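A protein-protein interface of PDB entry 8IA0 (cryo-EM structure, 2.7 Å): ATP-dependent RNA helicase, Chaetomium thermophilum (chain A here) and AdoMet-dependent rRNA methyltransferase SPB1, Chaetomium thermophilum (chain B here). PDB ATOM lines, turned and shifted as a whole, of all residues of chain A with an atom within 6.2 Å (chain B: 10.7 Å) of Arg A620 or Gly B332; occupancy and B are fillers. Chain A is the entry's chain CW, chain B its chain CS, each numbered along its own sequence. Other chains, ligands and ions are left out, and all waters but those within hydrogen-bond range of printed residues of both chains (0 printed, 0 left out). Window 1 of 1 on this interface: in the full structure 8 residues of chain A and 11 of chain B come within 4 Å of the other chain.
The backbone NH (N) of Gly B332 sits close to the guanidinium group (NH1) of Arg A620 (3.2 Å). O of Phe B331 sits close to OD1 of Asn A623 (2.8 Å). O of Ile B330 sits at hydrogen-bond distance from NH1 of Arg A620, at 2.4 Å.
OD1 of Asn A623 sits close to O of Val A619. O of Arg B328 is in hydrogen-bond range of N of Leu B333 (2.9 Å).
Ile A616 touches Ala B291. CD2 of Leu B295 touches CG2 of Ile A616, 3.9 Å away. Phe B331 touches Ile A616. Val A619 touches Phe B331 (CG1 to CG, 3.8 Å). Glu B329 touches Arg A620 (O to NH1, 3.98 Å). Arg A620 touches Phe B331. Val B287 touches Arg A622. OD1 of Asn A623 touches CD2 of Leu B333, at 3.96 Å.
Of the printed residues of chain B, Arg A622 touches Val B287. Of chain B, only Phe B331 and Leu B333 come within 4 Å of Asn A623. Gln A624 touches none of the printed residues of chain B. Of the printed residues of chain A, Ala B291 touches Ile A616. Of the printed residues of chain A, Glu B329 touches Arg A620. Printed residues of chain A within 4 Å of Phe B331: Ile A616 (3.5 Å), Val A619 (3.8 Å), Arg A620 (3.4 Å) and Asn A623 (2.8 Å). Gly B332 touches just one residue of chain A: Arg A620 (3.2 Å). Of the printed residues of chain A, Leu B333 touches Asn A623. The nearest printed residue of chain A that does not touch Leu B295 is Val A619 (8.2 Å).
Of the 19 printed residues of chain B, 8 touch a printed residue of chain A. Of the 9 printed residues of chain A, 5 touch a printed residue of chain B. Printed residues of chain A that touch a printed residue of chain B: Ile A616, Val A619, Arg A620, Arg A622 and Asn A623. Hydrophobic or aromatic side chains of chain A within 4 Å of the printed part of chain B: Ile A616 and Val A619. Among the printed residues, 11 pairs touch across the chains.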
ATOM      1  N   ILE A 616     -10.837   4.628 -13.388  1.00  0.00           N
ATOM      2  CA  ILE A 616     -10.497   3.209 -13.387  1.00  0.00           C
ATOM      3  C   ILE A 616      -9.046   2.959 -13.784  1.00  0.00           C
ATOM      4  O   ILE A 616      -8.482   1.919 -13.425  1.00  0.00           O
ATOM      5  CB  ILE A 616     -11.494   2.405 -14.247  1.00  0.00           C
ATOM      6  CG1 ILE A 616     -11.921   3.150 -15.520  1.00  0.00           C
ATOM      7  CG2 ILE A 616     -12.702   1.997 -13.424  1.00  0.00           C
ATOM      8  CD1 ILE A 616     -10.827   3.475 -16.498  1.00  0.00           C
ATOM      9  N   ASN A 617      -8.412   3.884 -14.511  1.00  0.00           N
ATOM     10  CA  ASN A 617      -7.016   3.678 -14.883  1.00  0.00           C
ATOM     11  C   ASN A 617      -6.111   3.647 -13.660  1.00  0.00           C
ATOM     12  O   ASN A 617      -5.127   2.900 -13.642  1.00  0.00           O
ATOM     13  CB  ASN A 617      -6.557   4.759 -15.858  1.00  0.00           C
ATOM     14  CG  ASN A 617      -7.155   6.102 -15.549  1.00  0.00           C
ATOM     15  OD1 ASN A 617      -7.839   6.265 -14.542  1.00  0.00           O
ATOM     16  ND2 ASN A 617      -6.898   7.081 -16.408  1.00  0.00           N
ATOM     17  N   GLU A 618      -6.424   4.443 -12.632  1.00  0.00           N
ATOM     18  CA  GLU A 618      -5.648   4.386 -11.397  1.00  0.00           C
ATOM     19  C   GLU A 618      -5.718   2.997 -10.779  1.00  0.00           C
ATOM     20  O   GLU A 618      -4.731   2.507 -10.216  1.00  0.00           O
ATOM     21  CB  GLU A 618      -6.148   5.434 -10.404  1.00  0.00           C
ATOM     22  CG  GLU A 618      -6.869   6.612 -11.030  1.00  0.00           C
ATOM     23  CD  GLU A 618      -7.275   7.653 -10.005  1.00  0.00           C
ATOM     24  OE1 GLU A 618      -6.526   7.847  -9.023  1.00  0.00           O
ATOM     25  OE2 GLU A 618      -8.342   8.277 -10.176  1.00  0.00           O
ATOM     26  N   VAL A 619      -6.883   2.354 -10.866  1.00  0.00           N
ATOM     27  CA  VAL A 619      -7.022   0.989 -10.370  1.00  0.00           C
ATOM     28  C   VAL A 619      -6.123   0.044 -11.156  1.00  0.00           C
ATOM     29  O   VAL A 619      -5.441  -0.811 -10.577  1.00  0.00           O
ATOM     30  CB  VAL A 619      -8.497   0.549 -10.428  1.00  0.00           C
ATOM     31  CG1 VAL A 619      -8.660  -0.853  -9.862  1.00  0.00           C
ATOM     32  CG2 VAL A 619      -9.376   1.544  -9.684  1.00  0.00           C
ATOM     33  N   ARG A 620      -6.102   0.184 -12.485  1.00  0.00           N
ATOM     34  CA  ARG A 620      -5.221  -0.649 -13.297  1.00  0.00           C
ATOM     35  C   ARG A 620      -3.757  -0.386 -12.972  1.00  0.00           C
ATOM     36  O   ARG A 620      -2.956  -1.324 -12.885  1.00  0.00           O
ATOM     37  CB  ARG A 620      -5.487  -0.414 -14.784  1.00  0.00           C
ATOM     38  CG  ARG A 620      -6.936  -0.123 -15.125  1.00  0.00           C
ATOM     39  CD  ARG A 620      -7.096   0.367 -16.564  1.00  0.00           C
ATOM     40  NE  ARG A 620      -6.376  -0.415 -17.567  1.00  0.00           N
ATOM     41  CZ  ARG A 620      -6.427  -1.734 -17.711  1.00  0.00           C
ATOM     42  NH1 ARG A 620      -7.236  -2.485 -16.981  1.00  0.00           N
ATOM     43  NH2 ARG A 620      -5.666  -2.314 -18.633  1.00  0.00           N
ATOM     44  N   LYS A 621      -3.386   0.884 -12.794  1.00  0.00           N
ATOM     45  CA  LYS A 621      -2.009   1.208 -12.433  1.00  0.00           C
ATOM     46  C   LYS A 621      -1.646   0.632 -11.071  1.00  0.00           C
ATOM     47  O   LYS A 621      -0.533   0.126 -10.879  1.00  0.00           O
ATOM     48  CB  LYS A 621      -1.803   2.724 -12.442  1.00  0.00           C
ATOM     49  CG  LYS A 621      -1.978   3.381 -13.802  1.00  0.00           C
ATOM     50  CD  LYS A 621      -0.920   2.914 -14.787  1.00  0.00           C
ATOM     51  CE  LYS A 621      -0.993   3.703 -16.083  1.00  0.00           C
ATOM     52  NZ  LYS A 621      -2.247   3.423 -16.836  1.00  0.00           N
ATOM     53  N   ARG A 622      -2.567   0.706 -10.109  1.00  0.00           N
ATOM     54  CA  ARG A 622      -2.289   0.176  -8.778  1.00  0.00           C
ATOM     55  C   ARG A 622      -2.141  -1.340  -8.804  1.00  0.00           C
ATOM     56  O   ARG A 622      -1.310  -1.900  -8.078  1.00  0.00           O
ATOM     57  CB  ARG A 622      -3.390   0.596  -7.806  1.00  0.00           C
ATOM     58  CG  ARG A 622      -3.089   0.279  -6.350  1.00  0.00           C
ATOM     59  CD  ARG A 622      -4.092   0.934  -5.408  1.00  0.00           C
ATOM     60  NE  ARG A 622      -4.051   2.391  -5.480  1.00  0.00           N
ATOM     61  CZ  ARG A 622      -4.905   3.135  -6.170  1.00  0.00           C
ATOM     62  NH1 ARG A 622      -5.892   2.593  -6.865  1.00  0.00           N
ATOM     63  NH2 ARG A 622      -4.765   4.458  -6.163  1.00  0.00           N
ATOM     64  N   ASN A 623      -2.941  -2.023  -9.627  1.00  0.00           N
ATOM     65  CA  ASN A 623      -2.839  -3.477  -9.715  1.00  0.00           C
ATOM     66  C   ASN A 623      -1.493  -3.908 -10.284  1.00  0.00           C
ATOM     67  O   ASN A 623      -0.889  -4.874  -9.804  1.00  0.00           O
ATOM     68  CB  ASN A 623      -3.985  -4.036 -10.557  1.00  0.00           C
ATOM     69  CG  ASN A 623      -5.344  -3.792  -9.929  1.00  0.00           C
ATOM     70  OD1 ASN A 623      -6.308  -3.456 -10.615  1.00  0.00           O
ATOM     71  ND2 ASN A 623      -5.425  -3.960  -8.614  1.00  0.00           N
ATOM     72  N   GLN A 624      -1.005  -3.208 -11.304  1.00  0.00           N
ATOM     73  CA  GLN A 624       0.280  -3.550 -11.906  1.00  0.00           C
ATOM     74  C   GLN A 624       1.429  -2.939 -11.112  1.00  0.00           C
ATOM     75  O   GLN A 624       1.599  -3.228  -9.928  1.00  0.00           O
ATOM     76  CB  GLN A 624       0.338  -3.087 -13.365  1.00  0.00           C
ATOM     77  CG  GLN A 624       0.127  -1.595 -13.563  1.00  0.00           C
ATOM     78  CD  GLN A 624       1.428  -0.817 -13.590  1.00  0.00           C
ATOM     79  OE1 GLN A 624       2.499  -1.384 -13.809  1.00  0.00           O
ATOM     80  NE2 GLN A 624       1.341   0.490 -13.368  1.00  0.00           N
ATOM     81  N   ILE B 262     -14.214  -9.186  -5.960  1.00  0.00           N
ATOM     82  CA  ILE B 262     -13.517  -9.040  -7.235  1.00  0.00           C
ATOM     83  C   ILE B 262     -12.125  -9.656  -7.159  1.00  0.00           C
ATOM     84  O   ILE B 262     -11.702 -10.389  -8.060  1.00  0.00           O
ATOM     85  CB  ILE B 262     -13.459  -7.560  -7.647  1.00  0.00           C
ATOM     86  CG1 ILE B 262     -14.871  -6.991  -7.791  1.00  0.00           C
ATOM     87  CG2 ILE B 262     -12.686  -7.399  -8.943  1.00  0.00           C
ATOM     88  CD1 ILE B 262     -15.689  -7.655  -8.871  1.00  0.00           C
ATOM     89  N   ASN B 263     -11.394  -9.379  -6.077  1.00  0.00           N
ATOM     90  CA  ASN B 263      -9.993  -9.772  -5.981  1.00  0.00           C
ATOM     91  C   ASN B 263      -9.778 -11.206  -5.515  1.00  0.00           C
ATOM     92  O   ASN B 263      -8.662 -11.717  -5.658  1.00  0.00           O
ATOM     93  CB  ASN B 263      -9.243  -8.833  -5.035  1.00  0.00           C
ATOM     94  CG  ASN B 263      -9.021  -7.462  -5.630  1.00  0.00           C
ATOM     95  OD1 ASN B 263      -9.018  -6.461  -4.920  1.00  0.00           O
ATOM     96  ND2 ASN B 263      -8.833  -7.410  -6.943  1.00  0.00           N
ATOM     97  N   VAL B 287     -11.017   3.807  -3.298  1.00  0.00           N
ATOM     98  CA  VAL B 287     -11.204   4.325  -4.649  1.00  0.00           C
ATOM     99  C   VAL B 287     -11.758   3.243  -5.567  1.00  0.00           C
ATOM    100  O   VAL B 287     -12.475   3.537  -6.532  1.00  0.00           O
ATOM    101  CB  VAL B 287      -9.889   4.924  -5.183  1.00  0.00           C
ATOM    102  CG1 VAL B 287      -9.212   5.755  -4.104  1.00  0.00           C
ATOM    103  CG2 VAL B 287      -8.948   3.835  -5.677  1.00  0.00           C
ATOM    104  N   ALA B 288     -11.438   1.978  -5.288  1.00  0.00           N
ATOM    105  CA  ALA B 288     -11.977   0.887  -6.092  1.00  0.00           C
ATOM    106  C   ALA B 288     -13.484   0.753  -5.902  1.00  0.00           C
ATOM    107  O   ALA B 288     -14.214   0.462  -6.855  1.00  0.00           O
ATOM    108  CB  ALA B 288     -11.265  -0.419  -5.748  1.00  0.00           C
ATOM    109  N   ALA B 291     -14.960   3.362  -8.007  1.00  0.00           N
ATOM    110  CA  ALA B 291     -14.928   2.960  -9.408  1.00  0.00           C
ATOM    111  C   ALA B 291     -15.947   1.865  -9.692  1.00  0.00           C
ATOM    112  O   ALA B 291     -16.703   1.950 -10.667  1.00  0.00           O
ATOM    113  CB  ALA B 291     -13.522   2.497  -9.788  1.00  0.00           C
ATOM    114  N   LEU B 292     -15.993   0.834  -8.844  1.00  0.00           N
ATOM    115  CA  LEU B 292     -16.895  -0.286  -9.092  1.00  0.00           C
ATOM    116  C   LEU B 292     -18.357   0.123  -8.960  1.00  0.00           C
ATOM    117  O   LEU B 292     -19.212  -0.415  -9.671  1.00  0.00           O
ATOM    118  CB  LEU B 292     -16.572  -1.439  -8.145  1.00  0.00           C
ATOM    119  CG  LEU B 292     -17.365  -2.732  -8.341  1.00  0.00           C
ATOM    120  CD1 LEU B 292     -17.339  -3.157  -9.796  1.00  0.00           C
ATOM    121  CD2 LEU B 292     -16.804  -3.830  -7.461  1.00  0.00           C
ATOM    122  N   LEU B 295     -19.417   1.989 -12.305  1.00  0.00           N
ATOM    123  CA  LEU B 295     -19.330   1.279 -13.569  1.00  0.00           C
ATOM    124  C   LEU B 295     -20.724   1.019 -14.137  1.00  0.00           C
ATOM    125  O   LEU B 295     -21.685   0.829 -13.388  1.00  0.00           O
ATOM    126  CB  LEU B 295     -18.590  -0.044 -13.396  1.00  0.00           C
ATOM    127  CG  LEU B 295     -17.073   0.001 -13.203  1.00  0.00           C
ATOM    128  CD1 LEU B 295     -16.431  -1.245 -13.789  1.00  0.00           C
ATOM    129  CD2 LEU B 295     -16.479   1.253 -13.834  1.00  0.00           C
ATOM    130  N   ARG B 324     -18.272 -10.309 -12.341  1.00  0.00           N
ATOM    131  CA  ARG B 324     -16.947 -10.267 -11.734  1.00  0.00           C
ATOM    132  C   ARG B 324     -15.855 -10.366 -12.790  1.00  0.00           C
ATOM    133  O   ARG B 324     -14.859  -9.637 -12.733  1.00  0.00           O
ATOM    134  CB  ARG B 324     -16.799 -11.394 -10.715  1.00  0.00           C
ATOM    135  CG  ARG B 324     -15.514 -11.327  -9.913  1.00  0.00           C
ATOM    136  CD  ARG B 324     -15.331 -12.571  -9.070  1.00  0.00           C
ATOM    137  NE  ARG B 324     -14.818 -13.689  -9.851  1.00  0.00           N
ATOM    138  CZ  ARG B 324     -13.555 -14.091  -9.837  1.00  0.00           C
ATOM    139  NH1 ARG B 324     -12.650 -13.495  -9.079  1.00  0.00           N
ATOM    140  NH2 ARG B 324     -13.194 -15.120 -10.597  1.00  0.00           N
ATOM    141  N   LEU B 325     -16.026 -11.268 -13.760  1.00  0.00           N
ATOM    142  CA  LEU B 325     -15.020 -11.430 -14.803  1.00  0.00           C
ATOM    143  C   LEU B 325     -14.915 -10.182 -15.669  1.00  0.00           C
ATOM    144  O   LEU B 325     -13.811  -9.772 -16.049  1.00  0.00           O
ATOM    145  CB  LEU B 325     -15.349 -12.651 -15.659  1.00  0.00           C
ATOM    146  CG  LEU B 325     -15.042 -14.011 -15.030  1.00  0.00           C
ATOM    147  CD1 LEU B 325     -15.141 -15.116 -16.065  1.00  0.00           C
ATOM    148  CD2 LEU B 325     -13.671 -14.003 -14.380  1.00  0.00           C
ATOM    149  N   ARG B 326     -16.053  -9.571 -15.998  1.00  0.00           N
ATOM    150  CA  ARG B 326     -16.038  -8.370 -16.826  1.00  0.00           C
ATOM    151  C   ARG B 326     -15.325  -7.226 -16.116  1.00  0.00           C
ATOM    152  O   ARG B 326     -14.564  -6.476 -16.737  1.00  0.00           O
ATOM    153  CB  ARG B 326     -17.468  -7.970 -17.187  1.00  0.00           C
ATOM    154  CG  ARG B 326     -17.584  -6.717 -18.040  1.00  0.00           C
ATOM    155  CD  ARG B 326     -17.146  -6.999 -19.471  1.00  0.00           C
ATOM    156  NE  ARG B 326     -15.847  -6.426 -19.804  1.00  0.00           N
ATOM    157  CZ  ARG B 326     -15.646  -5.152 -20.117  1.00  0.00           C
ATOM    158  NH1 ARG B 326     -16.638  -4.277 -20.128  1.00  0.00           N
ATOM    159  NH2 ARG B 326     -14.418  -4.749 -20.433  1.00  0.00           N
ATOM    160  N   VAL B 327     -15.564  -7.076 -14.811  1.00  0.00           N
ATOM    161  CA  VAL B 327     -14.911  -6.014 -14.051  1.00  0.00           C
ATOM    162  C   VAL B 327     -13.420  -6.292 -13.911  1.00  0.00           C
ATOM    163  O   VAL B 327     -12.594  -5.374 -13.998  1.00  0.00           O
ATOM    164  CB  VAL B 327     -15.592  -5.846 -12.680  1.00  0.00           C
ATOM    165  CG1 VAL B 327     -14.784  -4.919 -11.791  1.00  0.00           C
ATOM    166  CG2 VAL B 327     -17.001  -5.311 -12.855  1.00  0.00           C
ATOM    167  N   ARG B 328     -13.049  -7.557 -13.698  1.00  0.00           N
ATOM    168  CA  ARG B 328     -11.635  -7.901 -13.585  1.00  0.00           C
ATOM    169  C   ARG B 328     -10.891  -7.598 -14.879  1.00  0.00           C
ATOM    170  O   ARG B 328      -9.731  -7.169 -14.850  1.00  0.00           O
ATOM    171  CB  ARG B 328     -11.479  -9.372 -13.207  1.00  0.00           C
ATOM    172  CG  ARG B 328     -11.776  -9.669 -11.750  1.00  0.00           C
ATOM    173  CD  ARG B 328     -11.677 -11.154 -11.460  1.00  0.00           C
ATOM    174  NE  ARG B 328     -10.313 -11.650 -11.596  1.00  0.00           N
ATOM    175  CZ  ARG B 328      -9.430 -11.690 -10.609  1.00  0.00           C
ATOM    176  NH1 ARG B 328      -9.732 -11.261  -9.394  1.00  0.00           N
ATOM    177  NH2 ARG B 328      -8.215 -12.175 -10.845  1.00  0.00           N
ATOM    178  N   GLU B 329     -11.536  -7.824 -16.024  1.00  0.00           N
ATOM    179  CA  GLU B 329     -10.928  -7.455 -17.296  1.00  0.00           C
ATOM    180  C   GLU B 329     -10.726  -5.948 -17.392  1.00  0.00           C
ATOM    181  O   GLU B 329      -9.695  -5.483 -17.890  1.00  0.00           O
ATOM    182  CB  GLU B 329     -11.787  -7.961 -18.454  1.00  0.00           C
ATOM    183  CG  GLU B 329     -11.344  -9.304 -19.008  1.00  0.00           C
ATOM    184  CD  GLU B 329     -12.503 -10.129 -19.532  1.00  0.00           C
ATOM    185  OE1 GLU B 329     -13.612 -10.027 -18.966  1.00  0.00           O
ATOM    186  OE2 GLU B 329     -12.306 -10.881 -20.510  1.00  0.00           O
ATOM    187  N   ILE B 330     -11.705  -5.170 -16.927  1.00  0.00           N
ATOM    188  CA  ILE B 330     -11.560  -3.717 -16.911  1.00  0.00           C
ATOM    189  C   ILE B 330     -10.423  -3.309 -15.982  1.00  0.00           C
ATOM    190  O   ILE B 330      -9.590  -2.461 -16.323  1.00  0.00           O
ATOM    191  CB  ILE B 330     -12.884  -3.047 -16.502  1.00  0.00           C
ATOM    192  CG1 ILE B 330     -13.950  -3.262 -17.575  1.00  0.00           C
ATOM    193  CG2 ILE B 330     -12.680  -1.563 -16.251  1.00  0.00           C
ATOM    194  CD1 ILE B 330     -15.310  -2.725 -17.195  1.00  0.00           C
ATOM    195  N   PHE B 331     -10.366  -3.917 -14.799  1.00  0.00           N
ATOM    196  CA  PHE B 331      -9.388  -3.536 -13.789  1.00  0.00           C
ATOM    197  C   PHE B 331      -8.002  -4.110 -14.048  1.00  0.00           C
ATOM    198  O   PHE B 331      -7.060  -3.753 -13.332  1.00  0.00           O
ATOM    199  CB  PHE B 331      -9.872  -3.971 -12.404  1.00  0.00           C
ATOM    200  CG  PHE B 331     -10.956  -3.100 -11.836  1.00  0.00           C
ATOM    201  CD1 PHE B 331     -11.368  -1.961 -12.500  1.00  0.00           C
ATOM    202  CD2 PHE B 331     -11.563  -3.424 -10.636  1.00  0.00           C
ATOM    203  CE1 PHE B 331     -12.364  -1.162 -11.979  1.00  0.00           C
ATOM    204  CE2 PHE B 331     -12.559  -2.627 -10.110  1.00  0.00           C
ATOM    205  CZ  PHE B 331     -12.959  -1.496 -10.783  1.00  0.00           C
ATOM    206  N   GLY B 332      -7.848  -4.983 -15.038  1.00  0.00           N
ATOM    207  CA  GLY B 332      -6.544  -5.513 -15.375  1.00  0.00           C
ATOM    208  C   GLY B 332      -6.079  -6.686 -14.544  1.00  0.00           C
ATOM    209  O   GLY B 332      -4.878  -6.979 -14.537  1.00  0.00           O
ATOM    210  N   LEU B 333      -6.983  -7.363 -13.842  1.00  0.00           N
ATOM    211  CA  LEU B 333      -6.611  -8.548 -13.091  1.00  0.00           C
ATOM    212  C   LEU B 333      -6.200  -9.664 -14.051  1.00  0.00           C
ATOM    213  O   LEU B 333      -6.601  -9.666 -15.216  1.00  0.00           O
ATOM    214  CB  LEU B 333      -7.768  -9.002 -12.203  1.00  0.00           C
ATOM    215  CG  LEU B 333      -7.921  -8.324 -10.836  1.00  0.00           C
ATOM    216  CD1 LEU B 333      -6.654  -8.482 -10.009  1.00  0.00           C
ATOM    217  CD2 LEU B 333      -8.301  -6.856 -10.965  1.00  0.00           C
ATOM    218  N   PRO B 334      -5.371 -10.617 -13.581  1.00  0.00           N
ATOM    219  CA  PRO B 334      -4.817 -11.644 -14.479  1.00  0.00           C
ATOM    220  C   PRO B 334      -5.829 -12.301 -15.406  1.00  0.00           C
ATOM    221  O   PRO B 334      -5.722 -12.178 -16.630  1.00  0.00           O
ATOM    222  CB  PRO B 334      -4.229 -12.676 -13.509  1.00  0.00           C
ATOM    223  CG  PRO B 334      -4.010 -11.949 -12.220  1.00  0.00           C
ATOM    224  CD  PRO B 334      -4.709 -10.620 -12.266  1.00  0.00           C
ATOM    225  N   SER B 335      -6.815 -12.989 -14.843  1.00  0.00           N
ATOM    226  CA  SER B 335      -7.807 -13.684 -15.653  1.00  0.00           C
ATOM    227  C   SER B 335      -9.063 -13.988 -14.843  1.00  0.00           C
ATOM    228  O   SER B 335      -9.955 -13.147 -14.728  1.00  0.00           O
ATOM    229  CB  SER B 335      -7.221 -14.979 -16.222  1.00  0.00           C
ATOM    230  OG  SER B 335      -8.154 -15.632 -17.064  1.00  0.00           O
